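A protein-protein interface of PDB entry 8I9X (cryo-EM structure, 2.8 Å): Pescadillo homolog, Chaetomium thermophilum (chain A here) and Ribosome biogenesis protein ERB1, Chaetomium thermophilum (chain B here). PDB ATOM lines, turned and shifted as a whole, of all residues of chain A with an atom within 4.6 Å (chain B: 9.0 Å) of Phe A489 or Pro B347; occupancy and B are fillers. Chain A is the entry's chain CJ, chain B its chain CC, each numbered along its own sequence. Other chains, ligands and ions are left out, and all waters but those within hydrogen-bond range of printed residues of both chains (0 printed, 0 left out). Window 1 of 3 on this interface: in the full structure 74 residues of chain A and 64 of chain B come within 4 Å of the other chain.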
ATOM      1  N   PHE A 189      -7.000  16.803 -26.850  1.00  0.00           N
ATOM      2  CA  PHE A 189      -5.805  17.611 -26.637  1.00  0.00           C
ATOM      3  C   PHE A 189      -5.594  18.568 -27.800  1.00  0.00           C
ATOM      4  O   PHE A 189      -5.857  18.218 -28.953  1.00  0.00           O
ATOM      5  CB  PHE A 189      -4.582  16.710 -26.470  1.00  0.00           C
ATOM      6  CG  PHE A 189      -3.337  17.437 -26.046  1.00  0.00           C
ATOM      7  CD1 PHE A 189      -3.408  18.611 -25.322  1.00  0.00           C
ATOM      8  CD2 PHE A 189      -2.092  16.958 -26.409  1.00  0.00           C
ATOM      9  CE1 PHE A 189      -2.265  19.278 -24.949  1.00  0.00           C
ATOM     10  CE2 PHE A 189      -0.943  17.624 -26.040  1.00  0.00           C
ATOM     11  CZ  PHE A 189      -1.030  18.786 -25.311  1.00  0.00           C
ATOM     12  N   TYR A 196      -5.567  16.164 -30.939  1.00  0.00           N
ATOM     13  CA  TYR A 196      -5.462  14.748 -30.631  1.00  0.00           C
ATOM     14  C   TYR A 196      -6.751  14.271 -29.976  1.00  0.00           C
ATOM     15  O   TYR A 196      -7.261  14.912 -29.053  1.00  0.00           O
ATOM     16  CB  TYR A 196      -4.284  14.474 -29.694  1.00  0.00           C
ATOM     17  CG  TYR A 196      -2.924  14.559 -30.344  1.00  0.00           C
ATOM     18  CD1 TYR A 196      -2.380  13.472 -31.009  1.00  0.00           C
ATOM     19  CD2 TYR A 196      -2.172  15.721 -30.269  1.00  0.00           C
ATOM     20  CE1 TYR A 196      -1.134  13.544 -31.594  1.00  0.00           C
ATOM     21  CE2 TYR A 196      -0.925  15.803 -30.849  1.00  0.00           C
ATOM     22  CZ  TYR A 196      -0.411  14.712 -31.509  1.00  0.00           C
ATOM     23  OH  TYR A 196       0.832  14.790 -32.092  1.00  0.00           O
ATOM     24  N   GLN A 198      -8.483  10.777 -28.191  1.00  0.00           N
ATOM     25  CA  GLN A 198      -8.361   9.429 -27.657  1.00  0.00           C
ATOM     26  C   GLN A 198      -9.735   8.912 -27.259  1.00  0.00           C
ATOM     27  O   GLN A 198     -10.448   9.549 -26.476  1.00  0.00           O
ATOM     28  CB  GLN A 198      -7.434   9.386 -26.440  1.00  0.00           C
ATOM     29  CG  GLN A 198      -7.214   7.978 -25.908  1.00  0.00           C
ATOM     30  CD  GLN A 198      -6.252   7.932 -24.737  1.00  0.00           C
ATOM     31  OE1 GLN A 198      -5.763   8.961 -24.280  1.00  0.00           O
ATOM     32  NE2 GLN A 198      -5.978   6.730 -24.246  1.00  0.00           N
ATOM     33  N   LEU A 207      -6.038   6.468 -30.557  1.00  0.00           N
ATOM     34  CA  LEU A 207      -5.643   7.862 -30.668  1.00  0.00           C
ATOM     35  C   LEU A 207      -5.582   8.253 -32.138  1.00  0.00           C
ATOM     36  O   LEU A 207      -5.436   7.394 -33.009  1.00  0.00           O
ATOM     37  CB  LEU A 207      -4.286   8.091 -29.998  1.00  0.00           C
ATOM     38  CG  LEU A 207      -3.764   9.518 -29.838  1.00  0.00           C
ATOM     39  CD1 LEU A 207      -4.554  10.261 -28.775  1.00  0.00           C
ATOM     40  CD2 LEU A 207      -2.287   9.502 -29.493  1.00  0.00           C
ATOM     41  N   SER A 487      -1.576  18.354 -21.205  1.00  0.00           N
ATOM     42  CA  SER A 487      -1.848  17.184 -22.022  1.00  0.00           C
ATOM     43  C   SER A 487      -2.435  16.076 -21.153  1.00  0.00           C
ATOM     44  O   SER A 487      -1.832  15.692 -20.146  1.00  0.00           O
ATOM     45  CB  SER A 487      -0.578  16.679 -22.709  1.00  0.00           C
ATOM     46  OG  SER A 487       0.361  16.189 -21.774  1.00  0.00           O
ATOM     47  N   PRO A 488      -3.594  15.547 -21.506  1.00  0.00           N
ATOM     48  CA  PRO A 488      -4.163  14.446 -20.728  1.00  0.00           C
ATOM     49  C   PRO A 488      -3.623  13.098 -21.173  1.00  0.00           C
ATOM     50  O   PRO A 488      -4.384  12.144 -21.353  1.00  0.00           O
ATOM     51  CB  PRO A 488      -5.660  14.579 -21.009  1.00  0.00           C
ATOM     52  CG  PRO A 488      -5.699  15.055 -22.421  1.00  0.00           C
ATOM     53  CD  PRO A 488      -4.466  15.920 -22.634  1.00  0.00           C
ATOM     54  N   PHE A 489      -2.309  13.006 -21.353  1.00  0.00           N
ATOM     55  CA  PHE A 489      -1.684  11.776 -21.818  1.00  0.00           C
ATOM     56  C   PHE A 489      -0.470  11.350 -21.010  1.00  0.00           C
ATOM     57  O   PHE A 489      -0.135  10.160 -21.028  1.00  0.00           O
ATOM     58  CB  PHE A 489      -1.265  11.911 -23.289  1.00  0.00           C
ATOM     59  CG  PHE A 489      -2.407  12.188 -24.220  1.00  0.00           C
ATOM     60  CD1 PHE A 489      -3.476  11.315 -24.308  1.00  0.00           C
ATOM     61  CD2 PHE A 489      -2.412  13.323 -25.006  1.00  0.00           C
ATOM     62  CE1 PHE A 489      -4.525  11.572 -25.163  1.00  0.00           C
ATOM     63  CE2 PHE A 489      -3.458  13.582 -25.865  1.00  0.00           C
ATOM     64  CZ  PHE A 489      -4.516  12.707 -25.942  1.00  0.00           C
ATOM     65  N   VAL A 490       0.193  12.259 -20.309  1.00  0.00           N
ATOM     66  CA  VAL A 490       1.396  11.931 -19.557  1.00  0.00           C
ATOM     67  C   VAL A 490       0.993  11.425 -18.182  1.00  0.00           C
ATOM     68  O   VAL A 490       0.405  12.165 -17.384  1.00  0.00           O
ATOM     69  CB  VAL A 490       2.324  13.152 -19.448  1.00  0.00           C
ATOM     70  CG1 VAL A 490       3.534  12.823 -18.586  1.00  0.00           C
ATOM     71  CG2 VAL A 490       2.756  13.612 -20.829  1.00  0.00           C
ATOM     72  N   LYS A 491       1.305  10.166 -17.905  1.00  0.00           N
ATOM     73  CA  LYS A 491       1.022   9.617 -16.591  1.00  0.00           C
ATOM     74  C   LYS A 491       2.138   9.968 -15.617  1.00  0.00           C
ATOM     75  O   LYS A 491       3.292  10.136 -16.021  1.00  0.00           O
ATOM     76  CB  LYS A 491       0.863   8.097 -16.661  1.00  0.00           C
ATOM     77  CG  LYS A 491      -0.407   7.641 -17.356  1.00  0.00           C
ATOM     78  CD  LYS A 491      -1.633   8.292 -16.734  1.00  0.00           C
ATOM     79  CE  LYS A 491      -2.100   7.526 -15.507  1.00  0.00           C
ATOM     80  NZ  LYS A 491      -2.861   8.395 -14.567  1.00  0.00           N
ATOM     81  N   LYS B 344       4.061   1.807 -31.413  1.00  0.00           N
ATOM     82  CA  LYS B 344       3.109   2.905 -31.415  1.00  0.00           C
ATOM     83  C   LYS B 344       3.819   4.225 -31.141  1.00  0.00           C
ATOM     84  O   LYS B 344       4.833   4.277 -30.440  1.00  0.00           O
ATOM     85  CB  LYS B 344       2.013   2.671 -30.374  1.00  0.00           C
ATOM     86  CG  LYS B 344       1.079   1.524 -30.713  1.00  0.00           C
ATOM     87  CD  LYS B 344       0.061   1.298 -29.611  1.00  0.00           C
ATOM     88  CE  LYS B 344      -0.954   2.425 -29.563  1.00  0.00           C
ATOM     89  NZ  LYS B 344      -1.827   2.432 -30.769  1.00  0.00           N
ATOM     90  N   LEU B 345       3.282   5.295 -31.713  1.00  0.00           N
ATOM     91  CA  LEU B 345       3.867   6.610 -31.503  1.00  0.00           C
ATOM     92  C   LEU B 345       3.701   7.029 -30.044  1.00  0.00           C
ATOM     93  O   LEU B 345       2.674   6.729 -29.424  1.00  0.00           O
ATOM     94  CB  LEU B 345       3.214   7.639 -32.425  1.00  0.00           C
ATOM     95  CG  LEU B 345       3.609   7.563 -33.902  1.00  0.00           C
ATOM     96  CD1 LEU B 345       2.809   8.560 -34.726  1.00  0.00           C
ATOM     97  CD2 LEU B 345       5.100   7.799 -34.073  1.00  0.00           C
ATOM     98  N   PRO B 346       4.696   7.702 -29.464  1.00  0.00           N
ATOM     99  CA  PRO B 346       4.571   8.131 -28.074  1.00  0.00           C
ATOM    100  C   PRO B 346       3.427   9.115 -27.914  1.00  0.00           C
ATOM    101  O   PRO B 346       3.166   9.936 -28.810  1.00  0.00           O
ATOM    102  CB  PRO B 346       5.927   8.798 -27.784  1.00  0.00           C
ATOM    103  CG  PRO B 346       6.848   8.280 -28.831  1.00  0.00           C
ATOM    104  CD  PRO B 346       6.001   8.057 -30.040  1.00  0.00           C
ATOM    105  N   PRO B 347       2.692   9.045 -26.801  1.00  0.00           N
ATOM    106  CA  PRO B 347       1.637  10.012 -26.566  1.00  0.00           C
ATOM    107  C   PRO B 347       2.159  11.434 -26.658  1.00  0.00           C
ATOM    108  O   PRO B 347       3.355  11.689 -26.439  1.00  0.00           O
ATOM    109  CB  PRO B 347       1.194   9.685 -25.132  1.00  0.00           C
ATOM    110  CG  PRO B 347       1.359   8.137 -25.077  1.00  0.00           C
ATOM    111  CD  PRO B 347       2.195   7.744 -26.327  1.00  0.00           C
ATOM    112  N   PRO B 348       1.300  12.395 -26.987  1.00  0.00           N
ATOM    113  CA  PRO B 348       1.720  13.804 -26.968  1.00  0.00           C
ATOM    114  C   PRO B 348       2.091  14.250 -25.561  1.00  0.00           C
ATOM    115  O   PRO B 348       1.506  13.803 -24.572  1.00  0.00           O
ATOM    116  CB  PRO B 348       0.487  14.552 -27.488  1.00  0.00           C
ATOM    117  CG  PRO B 348      -0.385  13.513 -28.106  1.00  0.00           C
ATOM    118  CD  PRO B 348      -0.104  12.239 -27.395  1.00  0.00           C
ATOM    119  N   GLY B 349       3.065  15.149 -25.480  1.00  0.00           N
ATOM    120  CA  GLY B 349       3.572  15.641 -24.218  1.00  0.00           C
ATOM    121  C   GLY B 349       3.089  17.038 -23.888  1.00  0.00           C
ATOM    122  O   GLY B 349       2.280  17.637 -24.606  1.00  0.00           O
ATOM    123  N   TYR B 350       3.597  17.564 -22.777  1.00  0.00           N
ATOM    124  CA  TYR B 350       3.264  18.902 -22.304  1.00  0.00           C
ATOM    125  C   TYR B 350       3.872  20.003 -23.160  1.00  0.00           C
ATOM    126  O   TYR B 350       3.392  21.139 -23.112  1.00  0.00           O
ATOM    127  CB  TYR B 350       3.723  19.067 -20.851  1.00  0.00           C
ATOM    128  CG  TYR B 350       2.908  18.279 -19.853  1.00  0.00           C
ATOM    129  CD1 TYR B 350       1.527  18.236 -19.939  1.00  0.00           C
ATOM    130  CD2 TYR B 350       3.523  17.556 -18.841  1.00  0.00           C
ATOM    131  CE1 TYR B 350       0.778  17.513 -19.032  1.00  0.00           C
ATOM    132  CE2 TYR B 350       2.783  16.828 -17.935  1.00  0.00           C
ATOM    133  CZ  TYR B 350       1.411  16.809 -18.034  1.00  0.00           C
ATOM    134  OH  TYR B 350       0.665  16.087 -17.133  1.00  0.00           O
ATOM    135  N   ASP B 351       4.907  19.696 -23.940  1.00  0.00           N
ATOM    136  CA  ASP B 351       5.504  20.684 -24.828  1.00  0.00           C
ATOM    137  C   ASP B 351       4.600  21.052 -25.995  1.00  0.00           C
ATOM    138  O   ASP B 351       4.678  22.181 -26.489  1.00  0.00           O
ATOM    139  CB  ASP B 351       6.832  20.164 -25.381  1.00  0.00           C
ATOM    140  CG  ASP B 351       7.906  20.066 -24.325  1.00  0.00           C
ATOM    141  OD1 ASP B 351       7.861  20.857 -23.364  1.00  0.00           O
ATOM    142  OD2 ASP B 351       8.794  19.196 -24.455  1.00  0.00           O
ATOM    143  N   LEU B 352       3.752  20.132 -26.443  1.00  0.00           N
ATOM    144  CA  LEU B 352       3.041  20.288 -27.702  1.00  0.00           C
ATOM    145  C   LEU B 352       1.887  21.278 -27.643  1.00  0.00           C
ATOM    146  O   LEU B 352       1.579  21.895 -28.668  1.00  0.00           O
ATOM    147  CB  LEU B 352       2.518  18.931 -28.180  1.00  0.00           C
ATOM    148  CG  LEU B 352       3.579  18.005 -28.770  1.00  0.00           C
ATOM    149  CD1 LEU B 352       3.011  16.622 -29.027  1.00  0.00           C
ATOM    150  CD2 LEU B 352       4.137  18.600 -30.044  1.00  0.00           C
ATOM    151  N   LYS B 380      14.546  17.184 -31.132  1.00  0.00           N
ATOM    152  CA  LYS B 380      13.108  17.175 -31.332  1.00  0.00           C
ATOM    153  C   LYS B 380      12.765  18.045 -32.534  1.00  0.00           C
ATOM    154  O   LYS B 380      13.383  19.089 -32.761  1.00  0.00           O
ATOM    155  CB  LYS B 380      12.367  17.675 -30.088  1.00  0.00           C
ATOM    156  CG  LYS B 380      12.473  16.735 -28.900  1.00  0.00           C
ATOM    157  CD  LYS B 380      11.757  15.421 -29.154  1.00  0.00           C
ATOM    158  CE  LYS B 380      10.250  15.577 -29.069  1.00  0.00           C
ATOM    159  NZ  LYS B 380       9.569  14.261 -28.931  1.00  0.00           N
ATOM    160  N   TYR B 382      10.430  20.001 -33.123  1.00  0.00           N
ATOM    161  CA  TYR B 382       9.575  21.138 -32.825  1.00  0.00           C
ATOM    162  C   TYR B 382      10.083  21.849 -31.580  1.00  0.00           C
ATOM    163  O   TYR B 382      10.887  21.315 -30.812  1.00  0.00           O
ATOM    164  CB  TYR B 382       8.119  20.708 -32.626  1.00  0.00           C
ATOM    165  CG  TYR B 382       7.875  20.002 -31.314  1.00  0.00           C
ATOM    166  CD1 TYR B 382       8.181  18.659 -31.165  1.00  0.00           C
ATOM    167  CD2 TYR B 382       7.351  20.678 -30.223  1.00  0.00           C
ATOM    168  CE1 TYR B 382       7.963  18.006 -29.973  1.00  0.00           C
ATOM    169  CE2 TYR B 382       7.133  20.035 -29.023  1.00  0.00           C
ATOM    170  CZ  TYR B 382       7.441  18.697 -28.905  1.00  0.00           C
ATOM    171  OH  TYR B 382       7.226  18.041 -27.716  1.00  0.00           O
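Among the printed residues, pairs that only touch across the chains: Ser A487 with Tyr B350 (3.0 Å), Phe A489 with Pro B348 (3.5 Å), Tyr A196 with Pro B348 (3.5 Å), Phe A189 with Gly B349 (3.5 Å), Ser A487 with Gly B349 (3.6 Å), Phe A189 with Pro B348 (3.7 Å), Phe A489 with Pro B347 (3.8 Å), Ser A487 with Pro B348 (3.9 Å), Val A490 with Tyr B350 (3.9 Å) and Val A490 with Pro B348 (3.95 Å).
Of chain B, only Pro B347 (3.8 Å) and Pro B348 (3.5 Å) come within 4 Å of Phe A489. Pro B347 touches just one residue of chain A: Phe A489 (3.8 Å). Of the printed residues of chain B, Phe A189 touches Pro B348 (3.7 Å) and Gly B349 (3.5 Å). Of the printed residues of chain A, Tyr B350 touches Ser A487 (3.0 Å) and Val A490 (3.9 Å). Of the printed residues of chain A, Pro B348 touches Phe A189 (3.7 Å), Tyr A196 (3.5 Å), Ser A487 (3.9 Å), Phe A489 (3.5 Å) and Val A490 (3.95 Å). Of the printed residues of chain B, Ser A487 touches Pro B348 (3.9 Å), Gly B349 (3.6 Å) and Tyr B350 (3.0 Å). Tyr B382 touches none of the printed residues of chain A. The nearest printed residue of chain A that does not touch Gly B349 is Val A490 (4.03 Å).
N of Tyr A196 lies within hydrogen-bond range of O of Phe A189 (2.9 Å).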
